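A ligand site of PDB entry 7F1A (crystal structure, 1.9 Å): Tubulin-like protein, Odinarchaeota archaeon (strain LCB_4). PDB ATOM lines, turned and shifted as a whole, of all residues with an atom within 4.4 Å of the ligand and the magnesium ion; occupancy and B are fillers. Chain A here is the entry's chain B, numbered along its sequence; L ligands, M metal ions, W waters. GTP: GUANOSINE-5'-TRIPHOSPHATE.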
ATOM      1  N   GLY A  12      12.237 -14.060  -1.161  1.00  0.00           N
ATOM      2  CA  GLY A  12      12.523 -15.447  -1.493  1.00  0.00           C
ATOM      3  C   GLY A  12      13.997 -15.713  -1.836  1.00  0.00           C
ATOM      4  O   GLY A  12      14.848 -14.830  -1.771  1.00  0.00           O
ATOM      5  N   GLN A  13      14.286 -16.977  -2.183  1.00  0.00           N
ATOM      6  CA  GLN A  13      15.679 -17.385  -2.433  1.00  0.00           C
ATOM      7  C   GLN A  13      16.302 -16.547  -3.535  1.00  0.00           C
ATOM      8  O   GLN A  13      17.337 -15.903  -3.330  1.00  0.00           O
ATOM      9  CB  GLN A  13      15.777 -18.896  -2.762  1.00  0.00           C
ATOM     10  CG  GLN A  13      17.260 -19.360  -3.091  1.00  0.00           C
ATOM     11  CD  GLN A  13      17.569 -20.792  -2.603  1.00  0.00           C
ATOM     12  OE1 GLN A  13      16.670 -21.626  -2.542  1.00  0.00           O
ATOM     13  NE2 GLN A  13      18.828 -21.069  -2.251  1.00  0.00           N
ATOM     14  N   GLY A  14      15.675 -16.526  -4.711  1.00  0.00           N
ATOM     15  CA  GLY A  14      16.294 -15.810  -5.799  1.00  0.00           C
ATOM     16  C   GLY A  14      16.402 -14.326  -5.505  1.00  0.00           C
ATOM     17  O   GLY A  14      17.435 -13.696  -5.752  1.00  0.00           O
ATOM     18  N   GLN A  17      19.281 -13.752  -3.062  1.00  0.00           N
ATOM     19  CA  GLN A  17      20.566 -14.080  -3.670  1.00  0.00           C
ATOM     20  C   GLN A  17      20.964 -13.017  -4.691  1.00  0.00           C
ATOM     21  O   GLN A  17      22.122 -12.554  -4.698  1.00  0.00           O
ATOM     22  CB  GLN A  17      20.503 -15.503  -4.254  1.00  0.00           C
ATOM     23  CG  GLN A  17      20.540 -16.509  -3.082  1.00  0.00           C
ATOM     24  CD  GLN A  17      20.485 -17.950  -3.483  1.00  0.00           C
ATOM     25  OE1 GLN A  17      20.666 -18.827  -2.634  1.00  0.00           O
ATOM     26  NE2 GLN A  17      20.138 -18.221  -4.737  1.00  0.00           N
ATOM     27  N   ILE A  18      19.985 -12.513  -5.452  1.00  0.00           N
ATOM     28  CA  ILE A  18      20.230 -11.373  -6.350  1.00  0.00           C
ATOM     29  C   ILE A  18      20.670 -10.161  -5.539  1.00  0.00           C
ATOM     30  O   ILE A  18      21.546  -9.394  -5.968  1.00  0.00           O
ATOM     31  CB  ILE A  18      18.969 -11.085  -7.202  1.00  0.00           C
ATOM     32  CG1 ILE A  18      18.687 -12.252  -8.151  1.00  0.00           C
ATOM     33  CG2 ILE A  18      19.140  -9.809  -8.032  1.00  0.00           C
ATOM     34  CD1 ILE A  18      17.288 -12.190  -8.772  1.00  0.00           C
ATOM     35  N   ASP A  69      11.896 -13.611   3.459  1.00  0.00           N
ATOM     36  CA  ASP A  69      11.641 -14.967   2.965  1.00  0.00           C
ATOM     37  C   ASP A  69      10.741 -15.672   3.969  1.00  0.00           C
ATOM     38  O   ASP A  69      10.693 -15.295   5.148  1.00  0.00           O
ATOM     39  CB  ASP A  69      12.952 -15.736   2.762  1.00  0.00           C
ATOM     40  CG  ASP A  69      12.849 -16.875   1.716  1.00  0.00           C
ATOM     41  OD1 ASP A  69      11.756 -17.415   1.433  1.00  0.00           O
ATOM     42  OD2 ASP A  69      13.927 -17.228   1.148  1.00  0.00           O
ATOM     43  N   GLU A  71      11.279 -18.888   4.607  1.00  0.00           N
ATOM     44  CA  GLU A  71      12.188 -19.855   5.225  1.00  0.00           C
ATOM     45  C   GLU A  71      13.550 -19.213   5.396  1.00  0.00           C
ATOM     46  O   GLU A  71      13.873 -18.249   4.674  1.00  0.00           O
ATOM     47  CB  GLU A  71      12.298 -21.141   4.371  1.00  0.00           C
ATOM     48  CG  GLU A  71      13.042 -20.911   2.995  1.00  0.00           C
ATOM     49  CD  GLU A  71      14.544 -21.258   3.022  1.00  0.00           C
ATOM     50  OE1 GLU A  71      15.275 -20.783   2.116  1.00  0.00           O
ATOM     51  OE2 GLU A  71      14.992 -22.011   3.910  1.00  0.00           O
ATOM     52  N   GLY A  99       8.850 -22.558   4.260  1.00  0.00           N
ATOM     53  CA  GLY A  99       8.657 -21.869   3.008  1.00  0.00           C
ATOM     54  C   GLY A  99       7.212 -21.948   2.493  1.00  0.00           C
ATOM     55  O   GLY A  99       6.264 -22.326   3.185  1.00  0.00           O
ATOM     56  N   ALA A 100       7.065 -21.559   1.244  1.00  0.00           N
ATOM     57  CA  ALA A 100       5.785 -21.620   0.542  1.00  0.00           C
ATOM     58  C   ALA A 100       5.657 -22.887  -0.301  1.00  0.00           C
ATOM     59  O   ALA A 100       4.642 -23.074  -0.978  1.00  0.00           O
ATOM     60  CB  ALA A 100       5.618 -20.369  -0.330  1.00  0.00           C
ATOM     61  N   HIS A 101       6.682 -23.760  -0.287  1.00  0.00           N
ATOM     62  CA  HIS A 101       6.627 -25.054  -0.957  1.00  0.00           C
ATOM     63  C   HIS A 101       6.278 -24.908  -2.442  1.00  0.00           C
ATOM     64  O   HIS A 101       5.524 -25.729  -2.996  1.00  0.00           O
ATOM     65  CB  HIS A 101       5.630 -25.983  -0.265  1.00  0.00           C
ATOM     66  CG  HIS A 101       5.772 -26.030   1.221  1.00  0.00           C
ATOM     67  ND1 HIS A 101       6.998 -26.198   1.841  1.00  0.00           N
ATOM     68  CD2 HIS A 101       4.854 -25.948   2.219  1.00  0.00           C
ATOM     69  CE1 HIS A 101       6.825 -26.223   3.150  1.00  0.00           C
ATOM     70  NE2 HIS A 101       5.535 -26.064   3.408  1.00  0.00           N
ATOM     71  N   ASN A 102       6.780 -23.835  -3.064  1.00  0.00           N
ATOM     72  CA  ASN A 102       6.630 -23.518  -4.484  1.00  0.00           C
ATOM     73  C   ASN A 102       5.179 -23.258  -4.890  1.00  0.00           C
ATOM     74  O   ASN A 102       4.827 -23.422  -6.055  1.00  0.00           O
ATOM     75  CB  ASN A 102       7.186 -24.629  -5.389  1.00  0.00           C
ATOM     76  CG  ASN A 102       8.707 -24.594  -5.510  1.00  0.00           C
ATOM     77  OD1 ASN A 102       9.427 -23.709  -4.962  1.00  0.00           O
ATOM     78  ND2 ASN A 102       9.221 -25.580  -6.224  1.00  0.00           N
ATOM     79  N   THR A 138      11.909 -13.889  -7.841  1.00  0.00           N
ATOM     80  CA  THR A 138      11.596 -14.837  -8.899  1.00  0.00           C
ATOM     81  C   THR A 138      10.084 -15.096  -8.953  1.00  0.00           C
ATOM     82  O   THR A 138       9.367 -14.974  -7.955  1.00  0.00           O
ATOM     83  CB  THR A 138      12.329 -16.176  -8.694  1.00  0.00           C
ATOM     84  OG1 THR A 138      11.762 -16.873  -7.575  1.00  0.00           O
ATOM     85  CG2 THR A 138      13.858 -15.935  -8.479  1.00  0.00           C
ATOM     86  N   GLY A 141       8.945 -19.763  -8.133  1.00  0.00           N
ATOM     87  CA  GLY A 141       8.774 -20.390  -6.836  1.00  0.00           C
ATOM     88  C   GLY A 141       7.482 -19.918  -6.214  1.00  0.00           C
ATOM     89  O   GLY A 141       6.579 -19.461  -6.916  1.00  0.00           O
ATOM     90  N   GLY A 142       7.391 -20.030  -4.891  1.00  0.00           N
ATOM     91  CA  GLY A 142       6.157 -19.671  -4.189  1.00  0.00           C
ATOM     92  C   GLY A 142       6.248 -18.436  -3.294  1.00  0.00           C
ATOM     93  O   GLY A 142       5.245 -17.744  -3.099  1.00  0.00           O
ATOM     94  N   THR A 143       7.431 -18.116  -2.778  1.00  0.00           N
ATOM     95  CA  THR A 143       7.572 -16.960  -1.885  1.00  0.00           C
ATOM     96  C   THR A 143       7.823 -15.666  -2.679  1.00  0.00           C
ATOM     97  O   THR A 143       7.040 -14.705  -2.583  1.00  0.00           O
ATOM     98  CB  THR A 143       8.676 -17.216  -0.855  1.00  0.00           C
ATOM     99  OG1 THR A 143       8.207 -18.223   0.074  1.00  0.00           O
ATOM    100  CG2 THR A 143       9.006 -15.974  -0.071  1.00  0.00           C
ATOM    101  N   GLY A 144       8.859 -15.673  -3.504  1.00  0.00           N
ATOM    102  CA  GLY A 144       9.080 -14.549  -4.392  1.00  0.00           C
ATOM    103  C   GLY A 144       7.862 -14.262  -5.238  1.00  0.00           C
ATOM    104  O   GLY A 144       7.518 -13.088  -5.475  1.00  0.00           O
ATOM    105  N   VAL A 169      12.187 -12.508 -12.100  1.00  0.00           N
ATOM    106  CA  VAL A 169      12.855 -13.570 -12.846  1.00  0.00           C
ATOM    107  C   VAL A 169      11.837 -14.601 -13.324  1.00  0.00           C
ATOM    108  O   VAL A 169      11.262 -15.339 -12.526  1.00  0.00           O
ATOM    109  CB  VAL A 169      13.951 -14.249 -12.018  1.00  0.00           C
ATOM    110  CG1 VAL A 169      14.679 -15.264 -12.918  1.00  0.00           C
ATOM    111  CG2 VAL A 169      14.918 -13.200 -11.441  1.00  0.00           C
ATOM    112  N   ASP A 176      12.349 -25.261 -14.384  1.00  0.00           N
ATOM    113  CA  ASP A 176      12.912 -26.084 -13.316  1.00  0.00           C
ATOM    114  C   ASP A 176      12.019 -26.172 -12.076  1.00  0.00           C
ATOM    115  O   ASP A 176      12.480 -26.595 -11.011  1.00  0.00           O
ATOM    116  CB  ASP A 176      14.314 -25.577 -12.951  1.00  0.00           C
ATOM    117  CG  ASP A 176      14.310 -24.199 -12.353  1.00  0.00           C
ATOM    118  OD1 ASP A 176      13.500 -23.327 -12.745  1.00  0.00           O
ATOM    119  OD2 ASP A 176      15.199 -23.991 -11.466  1.00  0.00           O
ATOM    120  N   VAL A 177      10.793 -25.694 -12.163  1.00  0.00           N
ATOM    121  CA  VAL A 177       9.736 -25.948 -11.175  1.00  0.00           C
ATOM    122  C   VAL A 177       8.493 -26.268 -11.997  1.00  0.00           C
ATOM    123  O   VAL A 177       8.070 -25.437 -12.811  1.00  0.00           O
ATOM    124  CB  VAL A 177       9.485 -24.704 -10.289  1.00  0.00           C
ATOM    125  CG1 VAL A 177       8.270 -24.923  -9.384  1.00  0.00           C
ATOM    126  CG2 VAL A 177      10.747 -24.269  -9.531  1.00  0.00           C
ATOM    127  N   ASN A 203      16.499 -17.256 -16.757  1.00  0.00           N
ATOM    128  CA  ASN A 203      17.796 -17.898 -16.583  1.00  0.00           C
ATOM    129  C   ASN A 203      18.359 -18.509 -17.871  1.00  0.00           C
ATOM    130  O   ASN A 203      19.579 -18.684 -17.951  1.00  0.00           O
ATOM    131  CB  ASN A 203      17.689 -18.951 -15.506  1.00  0.00           C
ATOM    132  CG  ASN A 203      17.619 -18.338 -14.122  1.00  0.00           C
ATOM    133  OD1 ASN A 203      17.918 -17.138 -13.930  1.00  0.00           O
ATOM    134  ND2 ASN A 203      17.226 -19.136 -13.160  1.00  0.00           N
ATOM    135  N   LEU A 206      20.192 -15.586 -19.287  1.00  0.00           N
ATOM    136  CA  LEU A 206      21.339 -15.156 -18.475  1.00  0.00           C
ATOM    137  C   LEU A 206      22.511 -16.111 -18.630  1.00  0.00           C
ATOM    138  O   LEU A 206      23.664 -15.666 -18.745  1.00  0.00           O
ATOM    139  CB  LEU A 206      20.955 -15.031 -16.994  1.00  0.00           C
ATOM    140  CG  LEU A 206      19.897 -13.955 -16.692  1.00  0.00           C
ATOM    141  CD1 LEU A 206      19.426 -14.034 -15.263  1.00  0.00           C
ATOM    142  CD2 LEU A 206      20.380 -12.516 -17.072  1.00  0.00           C
ATOM    143  N   PHE A 222      24.989 -19.002  -8.139  1.00  0.00           N
ATOM    144  CA  PHE A 222      24.131 -18.026  -8.813  1.00  0.00           C
ATOM    145  C   PHE A 222      24.747 -16.642  -8.848  1.00  0.00           C
ATOM    146  O   PHE A 222      24.276 -15.795  -9.630  1.00  0.00           O
ATOM    147  CB  PHE A 222      22.783 -17.935  -8.135  1.00  0.00           C
ATOM    148  CG  PHE A 222      21.746 -18.833  -8.718  1.00  0.00           C
ATOM    149  CD1 PHE A 222      21.395 -18.739 -10.055  1.00  0.00           C
ATOM    150  CD2 PHE A 222      21.093 -19.752  -7.933  1.00  0.00           C
ATOM    151  CE1 PHE A 222      20.418 -19.565 -10.603  1.00  0.00           C
ATOM    152  CE2 PHE A 222      20.100 -20.572  -8.470  1.00  0.00           C
ATOM    153  CZ  PHE A 222      19.771 -20.481  -9.810  1.00  0.00           C
ATOM    154  N   LEU A 225      25.710 -15.406 -12.173  1.00  0.00           N
ATOM    155  CA  LEU A 225      24.548 -15.200 -13.026  1.00  0.00           C
ATOM    156  C   LEU A 225      23.843 -13.899 -12.625  1.00  0.00           C
ATOM    157  O   LEU A 225      23.510 -13.050 -13.463  1.00  0.00           O
ATOM    158  CB  LEU A 225      23.581 -16.369 -12.873  1.00  0.00           C
ATOM    159  CG  LEU A 225      22.824 -16.801 -14.120  1.00  0.00           C
ATOM    160  CD1 LEU A 225      23.836 -17.347 -15.114  1.00  0.00           C
ATOM    161  CD2 LEU A 225      21.764 -17.851 -13.774  1.00  0.00           C
ATOM    162  N   ASN A 226      23.581 -13.775 -11.331  1.00  0.00           N
ATOM    163  CA  ASN A 226      22.846 -12.635 -10.792  1.00  0.00           C
ATOM    164  C   ASN A 226      23.561 -11.306 -11.019  1.00  0.00           C
ATOM    165  O   ASN A 226      22.913 -10.255 -11.004  1.00  0.00           O
ATOM    166  CB  ASN A 226      22.613 -12.823  -9.294  1.00  0.00           C
ATOM    167  CG  ASN A 226      21.668 -13.977  -9.006  1.00  0.00           C
ATOM    168  OD1 ASN A 226      20.868 -14.358  -9.883  1.00  0.00           O
ATOM    169  ND2 ASN A 226      21.763 -14.540  -7.807  1.00  0.00           N
ATOM    170  N   ILE A 229      21.821  -9.022 -13.394  1.00  0.00           N
ATOM    171  CA  ILE A 229      20.654  -8.305 -12.868  1.00  0.00           C
ATOM    172  C   ILE A 229      21.088  -7.111 -12.021  1.00  0.00           C
ATOM    173  O   ILE A 229      20.507  -6.009 -12.115  1.00  0.00           O
ATOM    174  CB  ILE A 229      19.746  -9.275 -12.064  1.00  0.00           C
ATOM    175  CG1 ILE A 229      19.344 -10.479 -12.934  1.00  0.00           C
ATOM    176  CG2 ILE A 229      18.490  -8.524 -11.519  1.00  0.00           C
ATOM    177  CD1 ILE A 229      18.534 -11.598 -12.173  1.00  0.00           C
HETATM  178  PG  GTP L   1       9.697 -21.062  -2.105  1.00  0.00           P
HETATM  179  O1G GTP L   1       8.736 -21.853  -2.937  1.00  0.00           O
HETATM  180  O2G GTP L   1      11.081 -21.692  -2.028  1.00  0.00           O
HETATM  181  O3G GTP L   1       9.055 -20.822  -0.797  1.00  0.00           O
HETATM  182  O3B GTP L   1       9.815 -19.615  -2.854  1.00  0.00           O
HETATM  183  PB  GTP L   1      11.214 -18.936  -3.339  1.00  0.00           P
HETATM  184  O1B GTP L   1      10.755 -17.545  -3.644  1.00  0.00           O
HETATM  185  O2B GTP L   1      12.302 -18.907  -2.319  1.00  0.00           O
HETATM  186  O3A GTP L   1      11.611 -19.744  -4.671  1.00  0.00           O
HETATM  187  PA  GTP L   1      12.924 -19.615  -5.573  1.00  0.00           P
HETATM  188  O1A GTP L   1      13.470 -18.220  -5.386  1.00  0.00           O
HETATM  189  O2A GTP L   1      13.915 -20.707  -5.255  1.00  0.00           O
HETATM  190  O5' GTP L   1      12.325 -19.862  -7.041  1.00  0.00           O
HETATM  191  C5' GTP L   1      12.663 -20.918  -7.923  1.00  0.00           C
HETATM  192  C4' GTP L   1      12.988 -20.293  -9.288  1.00  0.00           C
HETATM  193  O4' GTP L   1      13.962 -19.260  -9.077  1.00  0.00           O
HETATM  194  C3' GTP L   1      13.606 -21.321 -10.215  1.00  0.00           C
HETATM  195  O3' GTP L   1      13.235 -21.012 -11.551  1.00  0.00           O
HETATM  196  C2' GTP L   1      15.085 -21.108  -9.913  1.00  0.00           C
HETATM  197  O2' GTP L   1      15.899 -21.574 -10.958  1.00  0.00           O
HETATM  198  C1' GTP L   1      15.149 -19.603  -9.747  1.00  0.00           C
HETATM  199  N9  GTP L   1      16.185 -19.053  -8.859  1.00  0.00           N
HETATM  200  C8  GTP L   1      16.332 -19.300  -7.511  1.00  0.00           C
HETATM  201  N7  GTP L   1      17.352 -18.523  -7.061  1.00  0.00           N
HETATM  202  C5  GTP L   1      17.806 -17.767  -8.097  1.00  0.00           C
HETATM  203  C6  GTP L   1      18.809 -16.817  -8.171  1.00  0.00           C
HETATM  204  O6  GTP L   1      19.466 -16.530  -7.166  1.00  0.00           O
HETATM  205  N1  GTP L   1      19.045 -16.183  -9.377  1.00  0.00           N
HETATM  206  C2  GTP L   1      18.319 -16.495 -10.490  1.00  0.00           C
HETATM  207  N2  GTP L   1      18.589 -15.865 -11.644  1.00  0.00           N
HETATM  208  N3  GTP L   1      17.309 -17.456 -10.421  1.00  0.00           N
HETATM  209  C4  GTP L   1      17.061 -18.062  -9.227  1.00  0.00           C
HETATM  210 MG    MG M   1      12.794 -20.724  -1.096  1.00  0.00          MG
HETATM  211  O   HOH W   1      11.343 -19.857   0.352  1.00  0.00           O
HETATM  212  O   HOH W   2      13.914 -21.447  -2.473  1.00  0.00           O
HETATM  213  O   HOH W   3      12.689 -15.157  -5.195  1.00  0.00           O
HETATM  214  O   HOH W   4      15.151 -21.355 -14.024  1.00  0.00           O
HETATM  215  O   HOH W   5      14.152 -19.647  -0.075  1.00  0.00           O
HETATM  216  O   HOH W   6       9.368 -17.350  -6.187  1.00  0.00           O
HETATM  217  O   HOH W   7      12.654 -23.282  -5.300  1.00  0.00           O
HETATM  218  O   HOH W   8      11.430 -18.153 -11.789  1.00  0.00           O
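Merely in contact with the magnesium ion: Gln 13 (3.9 Å). Of the 25 residues printed, 1 comes within 4 Å of the magnesium ion. The nearest printed residue that does not touch the magnesium ion is Glu 71 (4.1 Å).
Water W1 lies within hydrogen-bond range of the side-chain carboxylate of Asp 69 and an oxygen (O3G) of the ligand. Water W5 lies within hydrogen-bond range of OE1 of Glu 71 (2.7 Å), OD2 of Asp 69 (2.7 Å) and N of Gln 13 (3.4 Å). Water W7 bridges an oxygen (O2A) of the ligand (2.9 Å) and the side-chain amide oxygen (OD1) of Asn 102 (3.3 Å). Water W6 lies within hydrogen-bond range of OG1 of Thr 138 (2.8 Å), O1B of the ligand (2.9 Å), N of Gly 141 (3.1 Å) and N of Gly 144 (3.2 Å). Water W4 lies within hydrogen-bond range of the side-chain carboxylate of Asp 176 (2.9 Å), an oxygen (O3') of the ligand (3.1 Å) and the side-chain amide nitrogen of Asn 203 (3.2 Å). Water W3 lies within hydrogen-bond range of N of Thr 138 (3.0 Å), O1A of the ligand (3.2 Å) and N of Gly 14 (3.3 Å).
The magnesium ion is bound by water W2, water W5, an oxygen (O2G) of the ligand, water W1 and an oxygen (O2B) of the ligand.
OD2 of Asp 176 lies within hydrogen-bond range of O2' of the ligand (2.6 Å). A nitrogen (N1) of the ligand is in hydrogen-bond range of the side-chain amide oxygen (OD1) of Asn 226. O1B of the ligand is in hydrogen-bond range of N of Gly 144, 2.7 Å away. OD1 of Asn 203 is in hydrogen-bond range of N2 of the ligand. An oxygen (O2B) of the ligand lies close to the backbone NH (N) of Gln 13 (2.8 Å). An oxygen (O1G) of the ligand is in hydrogen-bond range of the backbone NH (N) of Asn 102, 2.8 Å away. The side-chain amide oxygen (OD1) of Asn 102 lies close to an oxygen (O1G) of the ligand (2.8 Å). An oxygen (O3B) of the ligand lies within hydrogen-bond range of the backbone NH (N) of Thr 143, at 2.8 Å. The side-chain hydroxyl (OG1) of Thr 143 is in hydrogen-bond range of an oxygen (O3G) of the ligand, 2.9 Å away. An oxygen (O1A) of the ligand sits at hydrogen-bond distance from the backbone NH (N) of Gly 14, 2.9 Å away. An oxygen (O3G) of the ligand is in hydrogen-bond range of the backbone NH (N) of Ala 100, 2.9 Å away. N of Gly 142 sits at hydrogen-bond distance from O1G of the ligand, 3.0 Å away. The side-chain amide nitrogen (NE2) of Gln 17 is in hydrogen-bond range of an oxygen (O6) of the ligand, 3.0 Å away. The side-chain hydroxyl (OG1) of Thr 138 is in hydrogen-bond range of an oxygen (O1A) of the ligand, 3.1 Å away.
ND2 of Asn 226 lies close to O of Phe 222. The side-chain amide nitrogen of Gln 13 sits at hydrogen-bond distance from the side-chain amide oxygen of Gln 17 (2.9 Å). The side-chain carboxylate (OD2) of Asp 69 sits at hydrogen-bond distance from the backbone NH (N) of Gln 13 (3.4 Å).
CA of Gly 12 touches O1B of the ligand, 3.5 Å away. Gly 99 touches the ligand (C to O3G, 3.9 Å). His 101 touches the ligand (N to O3G, 3.8 Å). N of Gly 141 touches O5' of the ligand, 3.6 Å away. Phe 222 touches the ligand. Within 4 Å of the ligand: Gly 12, Gln 13, Gly 14, Gln 17, Gly 99, Ala 100, His 101, Asn 102, Thr 138, Gly 141, Gly 142, Thr 143, Gly 144, Asp 176, Asn 203, Phe 222 and Asn 226. The nearest printed residue that does not touch the ligand is Asp 69 (4.1 Å).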
